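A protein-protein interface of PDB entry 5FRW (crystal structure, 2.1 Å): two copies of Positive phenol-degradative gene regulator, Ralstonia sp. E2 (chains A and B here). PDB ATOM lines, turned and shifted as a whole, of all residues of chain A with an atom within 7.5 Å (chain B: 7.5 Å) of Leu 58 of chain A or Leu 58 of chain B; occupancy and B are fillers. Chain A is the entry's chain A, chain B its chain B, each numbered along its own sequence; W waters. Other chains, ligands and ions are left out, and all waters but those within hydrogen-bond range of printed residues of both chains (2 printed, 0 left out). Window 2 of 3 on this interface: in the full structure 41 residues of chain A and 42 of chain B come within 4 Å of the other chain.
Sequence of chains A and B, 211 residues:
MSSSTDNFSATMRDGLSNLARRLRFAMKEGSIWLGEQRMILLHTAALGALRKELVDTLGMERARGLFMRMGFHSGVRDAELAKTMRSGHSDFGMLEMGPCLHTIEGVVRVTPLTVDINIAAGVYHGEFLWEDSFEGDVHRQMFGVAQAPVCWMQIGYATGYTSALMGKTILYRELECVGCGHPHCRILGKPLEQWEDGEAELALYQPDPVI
The side-chain hydroxyl (OG1) of Thr 57 of chain A sits at hydrogen-bond distance from the backbone carbonyl oxygen (O) of Glu 53 of chain A (3.2 Å).
The side-chain hydroxyl (OG1) of Thr 57 of chain B is in hydrogen-bond range of the backbone carbonyl oxygen (O) of Glu 53 of chain B (2.5 Å).
Water W1 lies within hydrogen-bond range of the backbone carbonyl oxygen of Leu 66 of chain A and the side-chain carboxylate of Glu 53 of chain B.
Water W2 lies within hydrogen-bond range of the backbone carbonyl oxygen of Leu 66 of chain B (2.9 Å) and the side-chain carboxylate of Glu 53 of chain A (2.9 Å).
Of the printed residues of chain B, Glu 53 of chain A touches Leu 66 (3.5 Å).
Of the printed residues of chain B, Leu 58 of chain A touches Leu 58 (3.7 Å).
No residue of chain B comes within 4 Å of Gly 59 of chain A.
Of the printed residues of chain B, Leu 66 of chain A touches Glu 53 (3.3 Å) and Leu 54 (3.9 Å).
Of the printed residues of chain A, Glu 53 of chain B touches Leu 66 (3.3 Å).
Of the printed residues of chain A, Leu 54 of chain B touches Leu 54 (3.9 Å) and Leu 66 (3.9 Å).
No residue of chain A comes within 4 Å of Gly 59 of chain B.
The nearest printed residue of chain B that does not touch Leu 54 of chain A is Leu 66 of chain B (4.4 Å).
Of the 14 printed residues of chain A, 4 touch a printed residue of chain B.
Hydrophobic or aromatic side chains of chain A that line the printed part of chain B: Leu 54, Leu 58 and Leu 66.
Along chain A the printed residues that touch a printed residue of chain B span positions 53 to 66.
Printed residues of chain B that touch a printed residue of chain A: Glu 53, Leu 54, Leu 58 and Leu 66.
Hydrophobic or aromatic side chains of chain B within 4 Å of the printed part of chain A: Leu 54, Leu 58 and Leu 66.
Among the printed residues, merely in contact across the chains: Leu 66 of chain A with Glu 53 of chain B (3.3 Å), Glu 53 of chain A with Leu 66 of chain B (3.5 Å), Leu 58 of chain A with Leu 58 of chain B (3.7 Å), Leu 66 of chain A with Leu 54 of chain B (3.9 Å) and Leu 54 of chain A with Leu 54 of chain B (3.9 Å).
Glu 53 of chain A touches Leu 66 of chain B, and with the chains exchanged Leu 66 of chain A touches Glu 53 of chain B.
Leu 54 of chain B touches its own counterpart, Leu 54 of chain A.
Leu 58 of chain A touches its own counterpart, Leu 58 of chain B.
Leu 66 of chain A touches Leu 54 of chain B, but with the chains exchanged Leu 54 of chain A does not touch Leu 66 of chain B (4.4 Å).
Positions printed for both chains: 52, 53, 54, 55, 56, 57, 58, 59, 60, 61, 62, 63, 64 and 66.
Of the 5 pairs that touch across the chains among the printed residues, 4 have their exchanged pair printed and touching as well.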
ATOM      1  N   LYS A  52      27.049 -28.101  14.612  1.00  0.00           N
ATOM      2  CA  LYS A  52      28.151 -28.031  13.657  1.00  0.00           C
ATOM      3  C   LYS A  52      28.169 -26.686  12.936  1.00  0.00           C
ATOM      4  O   LYS A  52      29.210 -26.037  12.861  1.00  0.00           O
ATOM      5  CB  LYS A  52      28.046 -29.176  12.649  1.00  0.00           C
ATOM      6  CG  LYS A  52      29.233 -29.327  11.687  1.00  0.00           C
ATOM      7  CD  LYS A  52      30.537 -29.658  12.433  1.00  0.00           C
ATOM      8  CE  LYS A  52      31.625 -30.199  11.490  1.00  0.00           C
ATOM      9  NZ  LYS A  52      32.852 -30.623  12.238  1.00  0.00           N
ATOM     10  N   GLU A  53      27.017 -26.243  12.435  1.00  0.00           N
ATOM     11  CA  GLU A  53      26.955 -24.973  11.704  1.00  0.00           C
ATOM     12  C   GLU A  53      27.186 -23.799  12.633  1.00  0.00           C
ATOM     13  O   GLU A  53      27.788 -22.793  12.247  1.00  0.00           O
ATOM     14  CB  GLU A  53      25.610 -24.791  10.993  1.00  0.00           C
ATOM     15  CG  GLU A  53      25.385 -25.709   9.804  1.00  0.00           C
ATOM     16  CD  GLU A  53      24.278 -25.222   8.870  1.00  0.00           C
ATOM     17  OE1 GLU A  53      24.327 -24.051   8.412  1.00  0.00           O
ATOM     18  OE2 GLU A  53      23.356 -26.022   8.589  1.00  0.00           O
ATOM     19  N   LEU A  54      26.676 -23.915  13.854  1.00  0.00           N
ATOM     20  CA  LEU A  54      26.852 -22.860  14.824  1.00  0.00           C
ATOM     21  C   LEU A  54      28.342 -22.692  15.167  1.00  0.00           C
ATOM     22  O   LEU A  54      28.864 -21.579  15.176  1.00  0.00           O
ATOM     23  CB  LEU A  54      26.009 -23.136  16.076  1.00  0.00           C
ATOM     24  CG  LEU A  54      24.515 -22.845  15.882  1.00  0.00           C
ATOM     25  CD1 LEU A  54      23.736 -22.946  17.170  1.00  0.00           C
ATOM     26  CD2 LEU A  54      24.302 -21.469  15.270  1.00  0.00           C
ATOM     27  N   VAL A  55      29.030 -23.791  15.433  1.00  0.00           N
ATOM     28  CA  VAL A  55      30.440 -23.693  15.781  1.00  0.00           C
ATOM     29  C   VAL A  55      31.247 -23.224  14.578  1.00  0.00           C
ATOM     30  O   VAL A  55      32.151 -22.398  14.716  1.00  0.00           O
ATOM     31  CB  VAL A  55      30.996 -25.033  16.288  1.00  0.00           C
ATOM     32  CG1 VAL A  55      32.515 -24.950  16.481  1.00  0.00           C
ATOM     33  CG2 VAL A  55      30.302 -25.425  17.585  1.00  0.00           C
ATOM     34  N   ASP A  56      30.890 -23.734  13.397  1.00  0.00           N
ATOM     35  CA  ASP A  56      31.612 -23.407  12.175  1.00  0.00           C
ATOM     36  C   ASP A  56      31.481 -21.941  11.789  1.00  0.00           C
ATOM     37  O   ASP A  56      32.433 -21.359  11.295  1.00  0.00           O
ATOM     38  CB  ASP A  56      31.150 -24.293  11.007  1.00  0.00           C
ATOM     39  CG  ASP A  56      31.824 -25.648  11.012  1.00  0.00           C
ATOM     40  OD1 ASP A  56      32.755 -25.862  11.821  1.00  0.00           O
ATOM     41  OD2 ASP A  56      31.435 -26.504  10.200  1.00  0.00           O
ATOM     42  N   THR A  57      30.329 -21.323  12.016  1.00  0.00           N
ATOM     43  CA  THR A  57      30.182 -19.932  11.585  1.00  0.00           C
ATOM     44  C   THR A  57      30.163 -18.907  12.716  1.00  0.00           C
ATOM     45  O   THR A  57      30.258 -17.713  12.456  1.00  0.00           O
ATOM     46  CB  THR A  57      28.902 -19.726  10.759  1.00  0.00           C
ATOM     47  OG1 THR A  57      27.775 -19.694  11.635  1.00  0.00           O
ATOM     48  CG2 THR A  57      28.721 -20.840   9.758  1.00  0.00           C
ATOM     49  N   LEU A  58      30.025 -19.349  13.961  1.00  0.00           N
ATOM     50  CA  LEU A  58      30.014 -18.407  15.075  1.00  0.00           C
ATOM     51  C   LEU A  58      31.239 -18.562  15.969  1.00  0.00           C
ATOM     52  O   LEU A  58      31.586 -17.641  16.704  1.00  0.00           O
ATOM     53  CB  LEU A  58      28.750 -18.565  15.921  1.00  0.00           C
ATOM     54  CG  LEU A  58      27.401 -18.324  15.250  1.00  0.00           C
ATOM     55  CD1 LEU A  58      26.290 -18.226  16.291  1.00  0.00           C
ATOM     56  CD2 LEU A  58      27.465 -17.061  14.428  1.00  0.00           C
ATOM     57  N   GLY A  59      31.877 -19.730  15.911  1.00  0.00           N
ATOM     58  CA  GLY A  59      32.983 -20.051  16.800  1.00  0.00           C
ATOM     59  C   GLY A  59      32.523 -20.916  17.964  1.00  0.00           C
ATOM     60  O   GLY A  59      31.338 -20.910  18.290  1.00  0.00           O
ATOM     61  N   MET A  60      33.442 -21.641  18.600  1.00  0.00           N
ATOM     62  CA  MET A  60      33.059 -22.587  19.643  1.00  0.00           C
ATOM     63  C   MET A  60      32.527 -21.887  20.907  1.00  0.00           C
ATOM     64  O   MET A  60      31.606 -22.389  21.554  1.00  0.00           O
ATOM     65  CB  MET A  60      34.240 -23.502  20.001  1.00  0.00           C
ATOM     66  CG  MET A  60      33.873 -24.990  20.052  1.00  0.00           C
ATOM     67  SD  MET A  60      35.224 -26.123  20.466  1.00  0.00           S
ATOM     68  CE  MET A  60      36.113 -26.291  18.921  1.00  0.00           C
ATOM     69  N   GLU A  61      33.082 -20.723  21.239  1.00  0.00           N
ATOM     70  CA  GLU A  61      32.714 -20.023  22.466  1.00  0.00           C
ATOM     71  C   GLU A  61      31.298 -19.453  22.415  1.00  0.00           C
ATOM     72  O   GLU A  61      30.519 -19.612  23.351  1.00  0.00           O
ATOM     73  CB  GLU A  61      33.713 -18.899  22.761  1.00  0.00           C
ATOM     74  CG  GLU A  61      34.585 -19.160  23.990  1.00  0.00           C
ATOM     75  CD  GLU A  61      33.926 -18.716  25.303  1.00  0.00           C
ATOM     76  OE1 GLU A  61      33.564 -17.518  25.440  1.00  0.00           O
ATOM     77  OE2 GLU A  61      33.765 -19.575  26.201  1.00  0.00           O
ATOM     78  N   ARG A  62      30.958 -18.789  21.321  1.00  0.00           N
ATOM     79  CA  ARG A  62      29.634 -18.198  21.205  1.00  0.00           C
ATOM     80  C   ARG A  62      28.554 -19.259  21.012  1.00  0.00           C
ATOM     81  O   ARG A  62      27.436 -19.116  21.542  1.00  0.00           O
ATOM     82  CB  ARG A  62      29.619 -17.179  20.073  1.00  0.00           C
ATOM     83  CG  ARG A  62      30.328 -15.880  20.490  1.00  0.00           C
ATOM     84  CD  ARG A  62      30.518 -14.932  19.326  1.00  0.00           C
ATOM     85  NE  ARG A  62      29.449 -15.069  18.341  1.00  0.00           N
ATOM     86  CZ  ARG A  62      28.355 -14.311  18.322  1.00  0.00           C
ATOM     87  NH1 ARG A  62      28.172 -13.372  19.252  1.00  0.00           N
ATOM     88  NH2 ARG A  62      27.433 -14.506  17.387  1.00  0.00           N
ATOM     89  N   ALA A  63      28.906 -20.329  20.297  1.00  0.00           N
ATOM     90  CA  ALA A  63      28.039 -21.491  20.140  1.00  0.00           C
ATOM     91  C   ALA A  63      27.793 -22.190  21.475  1.00  0.00           C
ATOM     92  O   ALA A  63      26.677 -22.645  21.748  1.00  0.00           O
ATOM     93  CB  ALA A  63      28.642 -22.486  19.135  1.00  0.00           C
ATOM     94  N   ARG A  64      28.836 -22.294  22.291  1.00  0.00           N
ATOM     95  CA  ARG A  64      28.685 -22.856  23.626  1.00  0.00           C
ATOM     96  C   ARG A  64      27.687 -22.043  24.441  1.00  0.00           C
ATOM     97  O   ARG A  64      26.889 -22.606  25.184  1.00  0.00           O
ATOM     98  CB  ARG A  64      30.022 -22.922  24.371  1.00  0.00           C
ATOM     99  CG  ARG A  64      29.841 -23.032  25.887  1.00  0.00           C
ATOM    100  CD  ARG A  64      31.071 -23.527  26.626  1.00  0.00           C
ATOM    101  NE  ARG A  64      32.160 -22.561  26.623  1.00  0.00           N
ATOM    102  CZ  ARG A  64      32.806 -22.176  27.719  1.00  0.00           C
ATOM    103  NH1 ARG A  64      32.452 -22.660  28.908  1.00  0.00           N
ATOM    104  NH2 ARG A  64      33.793 -21.294  27.631  1.00  0.00           N
ATOM    105  N   LEU A  66      25.087 -20.087  23.322  1.00  0.00           N
ATOM    106  CA  LEU A  66      23.740 -20.345  22.814  1.00  0.00           C
ATOM    107  C   LEU A  66      23.129 -21.629  23.367  1.00  0.00           C
ATOM    108  O   LEU A  66      21.932 -21.679  23.668  1.00  0.00           O
ATOM    109  CB  LEU A  66      23.748 -20.422  21.288  1.00  0.00           C
ATOM    110  CG  LEU A  66      23.793 -19.097  20.530  1.00  0.00           C
ATOM    111  CD1 LEU A  66      24.145 -19.380  19.080  1.00  0.00           C
ATOM    112  CD2 LEU A  66      22.454 -18.371  20.636  1.00  0.00           C
ATOM    113  N   LYS B  52      15.026 -16.919  18.803  1.00  0.00           N
ATOM    114  CA  LYS B  52      15.051 -15.464  18.969  1.00  0.00           C
ATOM    115  C   LYS B  52      16.496 -14.933  18.953  1.00  0.00           C
ATOM    116  O   LYS B  52      16.789 -13.936  18.298  1.00  0.00           O
ATOM    117  CB  LYS B  52      14.339 -15.040  20.263  1.00  0.00           C
ATOM    118  CG  LYS B  52      14.362 -13.514  20.495  1.00  0.00           C
ATOM    119  CD  LYS B  52      13.459 -13.077  21.624  1.00  0.00           C
ATOM    120  CE  LYS B  52      13.435 -11.549  21.730  1.00  0.00           C
ATOM    121  NZ  LYS B  52      12.831 -10.931  20.512  1.00  0.00           N
ATOM    122  N   GLU B  53      17.399 -15.617  19.647  1.00  0.00           N
ATOM    123  CA  GLU B  53      18.800 -15.218  19.643  1.00  0.00           C
ATOM    124  C   GLU B  53      19.413 -15.280  18.246  1.00  0.00           C
ATOM    125  O   GLU B  53      20.147 -14.365  17.837  1.00  0.00           O
ATOM    126  CB  GLU B  53      19.613 -16.093  20.594  1.00  0.00           C
ATOM    127  CG  GLU B  53      19.398 -15.794  22.069  1.00  0.00           C
ATOM    128  CD  GLU B  53      20.543 -16.307  22.917  1.00  0.00           C
ATOM    129  OE1 GLU B  53      21.696 -15.893  22.673  1.00  0.00           O
ATOM    130  OE2 GLU B  53      20.293 -17.127  23.822  1.00  0.00           O
ATOM    131  N   LEU B  54      19.118 -16.361  17.520  1.00  0.00           N
ATOM    132  CA  LEU B  54      19.619 -16.528  16.160  1.00  0.00           C
ATOM    133  C   LEU B  54      19.054 -15.454  15.230  1.00  0.00           C
ATOM    134  O   LEU B  54      19.789 -14.891  14.419  1.00  0.00           O
ATOM    135  CB  LEU B  54      19.289 -17.930  15.620  1.00  0.00           C
ATOM    136  CG  LEU B  54      20.010 -19.102  16.292  1.00  0.00           C
ATOM    137  CD1 LEU B  54      19.656 -20.422  15.614  1.00  0.00           C
ATOM    138  CD2 LEU B  54      21.519 -18.895  16.300  1.00  0.00           C
ATOM    139  N   VAL B  55      17.759 -15.164  15.342  1.00  0.00           N
ATOM    140  CA  VAL B  55      17.150 -14.106  14.528  1.00  0.00           C
ATOM    141  C   VAL B  55      17.702 -12.725  14.923  1.00  0.00           C
ATOM    142  O   VAL B  55      18.035 -11.911  14.059  1.00  0.00           O
ATOM    143  CB  VAL B  55      15.596 -14.104  14.636  1.00  0.00           C
ATOM    144  CG1 VAL B  55      15.008 -12.839  14.012  1.00  0.00           C
ATOM    145  CG2 VAL B  55      15.012 -15.328  13.942  1.00  0.00           C
ATOM    146  N   ASP B  56      17.822 -12.472  16.225  1.00  0.00           N
ATOM    147  CA  ASP B  56      18.318 -11.180  16.708  1.00  0.00           C
ATOM    148  C   ASP B  56      19.757 -10.907  16.274  1.00  0.00           C
ATOM    149  O   ASP B  56      20.078  -9.800  15.858  1.00  0.00           O
ATOM    150  CB  ASP B  56      18.216 -11.100  18.229  1.00  0.00           C
ATOM    151  CG  ASP B  56      16.787 -10.873  18.707  1.00  0.00           C
ATOM    152  OD1 ASP B  56      15.919 -10.531  17.872  1.00  0.00           O
ATOM    153  OD2 ASP B  56      16.531 -11.039  19.918  1.00  0.00           O
ATOM    154  N   THR B  57      20.609 -11.921  16.329  1.00  0.00           N
ATOM    155  CA  THR B  57      22.031 -11.712  16.115  1.00  0.00           C
ATOM    156  C   THR B  57      22.468 -11.990  14.677  1.00  0.00           C
ATOM    157  O   THR B  57      23.396 -11.359  14.169  1.00  0.00           O
ATOM    158  CB  THR B  57      22.849 -12.585  17.071  1.00  0.00           C
ATOM    159  OG1 THR B  57      22.442 -13.941  16.918  1.00  0.00           O
ATOM    160  CG2 THR B  57      22.603 -12.168  18.519  1.00  0.00           C
ATOM    161  N   LEU B  58      21.797 -12.921  14.009  1.00  0.00           N
ATOM    162  CA  LEU B  58      22.199 -13.285  12.664  1.00  0.00           C
ATOM    163  C   LEU B  58      21.181 -12.862  11.604  1.00  0.00           C
ATOM    164  O   LEU B  58      21.393 -13.103  10.434  1.00  0.00           O
ATOM    165  CB  LEU B  58      22.446 -14.792  12.580  1.00  0.00           C
ATOM    166  CG  LEU B  58      23.339 -15.500  13.598  1.00  0.00           C
ATOM    167  CD1 LEU B  58      23.512 -16.966  13.211  1.00  0.00           C
ATOM    168  CD2 LEU B  58      24.673 -14.806  13.655  1.00  0.00           C
ATOM    169  N   GLY B  59      20.081 -12.235  11.999  1.00  0.00           N
ATOM    170  CA  GLY B  59      19.060 -11.837  11.039  1.00  0.00           C
ATOM    171  C   GLY B  59      18.164 -12.988  10.602  1.00  0.00           C
ATOM    172  O   GLY B  59      18.568 -14.147  10.658  1.00  0.00           O
ATOM    173  N   MET B  60      16.956 -12.662  10.140  1.00  0.00           N
ATOM    174  CA  MET B  60      15.924 -13.668   9.883  1.00  0.00           C
ATOM    175  C   MET B  60      16.270 -14.634   8.764  1.00  0.00           C
ATOM    176  O   MET B  60      16.017 -15.822   8.892  1.00  0.00           O
ATOM    177  CB  MET B  60      14.576 -12.998   9.580  1.00  0.00           C
ATOM    178  CG  MET B  60      13.374 -13.864   9.970  1.00  0.00           C
ATOM    179  SD  MET B  60      11.820 -12.980  10.190  1.00  0.00           S
ATOM    180  CE  MET B  60      12.174 -11.943  11.597  1.00  0.00           C
ATOM    181  N   GLU B  61      16.858 -14.141   7.679  1.00  0.00           N
ATOM    182  CA  GLU B  61      17.134 -14.988   6.517  1.00  0.00           C
ATOM    183  C   GLU B  61      18.158 -16.081   6.800  1.00  0.00           C
ATOM    184  O   GLU B  61      18.004 -17.213   6.363  1.00  0.00           O
ATOM    185  CB  GLU B  61      17.601 -14.137   5.342  1.00  0.00           C
ATOM    186  CG  GLU B  61      16.636 -14.177   4.173  1.00  0.00           C
ATOM    187  CD  GLU B  61      16.916 -13.095   3.151  1.00  0.00           C
ATOM    188  OE1 GLU B  61      18.106 -12.856   2.842  1.00  0.00           O
ATOM    189  OE2 GLU B  61      15.942 -12.478   2.666  1.00  0.00           O
ATOM    190  N   ARG B  62      19.198 -15.721   7.531  1.00  0.00           N
ATOM    191  CA  ARG B  62      20.215 -16.655   7.978  1.00  0.00           C
ATOM    192  C   ARG B  62      19.677 -17.644   9.031  1.00  0.00           C
ATOM    193  O   ARG B  62      20.010 -18.822   9.011  1.00  0.00           O
ATOM    194  CB  ARG B  62      21.395 -15.844   8.497  1.00  0.00           C
ATOM    195  CG  ARG B  62      22.120 -15.074   7.491  1.00  0.00           C
ATOM    196  CD  ARG B  62      23.281 -14.361   8.111  1.00  0.00           C
ATOM    197  NE  ARG B  62      23.953 -13.540   7.110  1.00  0.00           N
ATOM    198  CZ  ARG B  62      24.956 -12.694   7.381  1.00  0.00           C
ATOM    199  NH1 ARG B  62      25.433 -12.537   8.621  1.00  0.00           N
ATOM    200  NH2 ARG B  62      25.475 -11.982   6.402  1.00  0.00           N
ATOM    201  N   ALA B  63      18.822 -17.162   9.928  1.00  0.00           N
ATOM    202  CA  ALA B  63      18.191 -18.016  10.935  1.00  0.00           C
ATOM    203  C   ALA B  63      17.219 -19.010  10.294  1.00  0.00           C
ATOM    204  O   ALA B  63      17.133 -20.166  10.708  1.00  0.00           O
ATOM    205  CB  ALA B  63      17.466 -17.166  11.956  1.00  0.00           C
ATOM    206  N   ARG B  64      16.493 -18.536   9.289  1.00  0.00           N
ATOM    207  CA  ARG B  64      15.582 -19.364   8.524  1.00  0.00           C
ATOM    208  C   ARG B  64      16.343 -20.542   7.895  1.00  0.00           C
ATOM    209  O   ARG B  64      15.908 -21.691   7.991  1.00  0.00           O
ATOM    210  CB  ARG B  64      14.876 -18.517   7.456  1.00  0.00           C
ATOM    211  CG  ARG B  64      13.889 -19.268   6.571  1.00  0.00           C
ATOM    212  CD  ARG B  64      12.946 -18.297   5.862  1.00  0.00           C
ATOM    213  NE  ARG B  64      13.656 -17.421   4.933  1.00  0.00           N
ATOM    214  CZ  ARG B  64      13.711 -17.608   3.616  1.00  0.00           C
ATOM    215  NH1 ARG B  64      13.087 -18.644   3.061  1.00  0.00           N
ATOM    216  NH2 ARG B  64      14.392 -16.758   2.855  1.00  0.00           N
ATOM    217  N   LEU B  66      19.349 -21.955   8.781  1.00  0.00           N
ATOM    218  CA  LEU B  66      19.769 -22.875   9.841  1.00  0.00           C
ATOM    219  C   LEU B  66      18.656 -23.845  10.257  1.00  0.00           C
ATOM    220  O   LEU B  66      18.896 -25.029  10.437  1.00  0.00           O
ATOM    221  CB  LEU B  66      20.230 -22.080  11.070  1.00  0.00           C
ATOM    222  CG  LEU B  66      21.475 -21.232  10.864  1.00  0.00           C
ATOM    223  CD1 LEU B  66      21.661 -20.205  11.986  1.00  0.00           C
ATOM    224  CD2 LEU B  66      22.655 -22.170  10.774  1.00  0.00           C
HETATM  225  O   HOH W   1      19.797 -19.994  23.211  1.00  0.00           O
HETATM  226  O   HOH W   2      21.482 -26.173  10.824  1.00  0.00           O
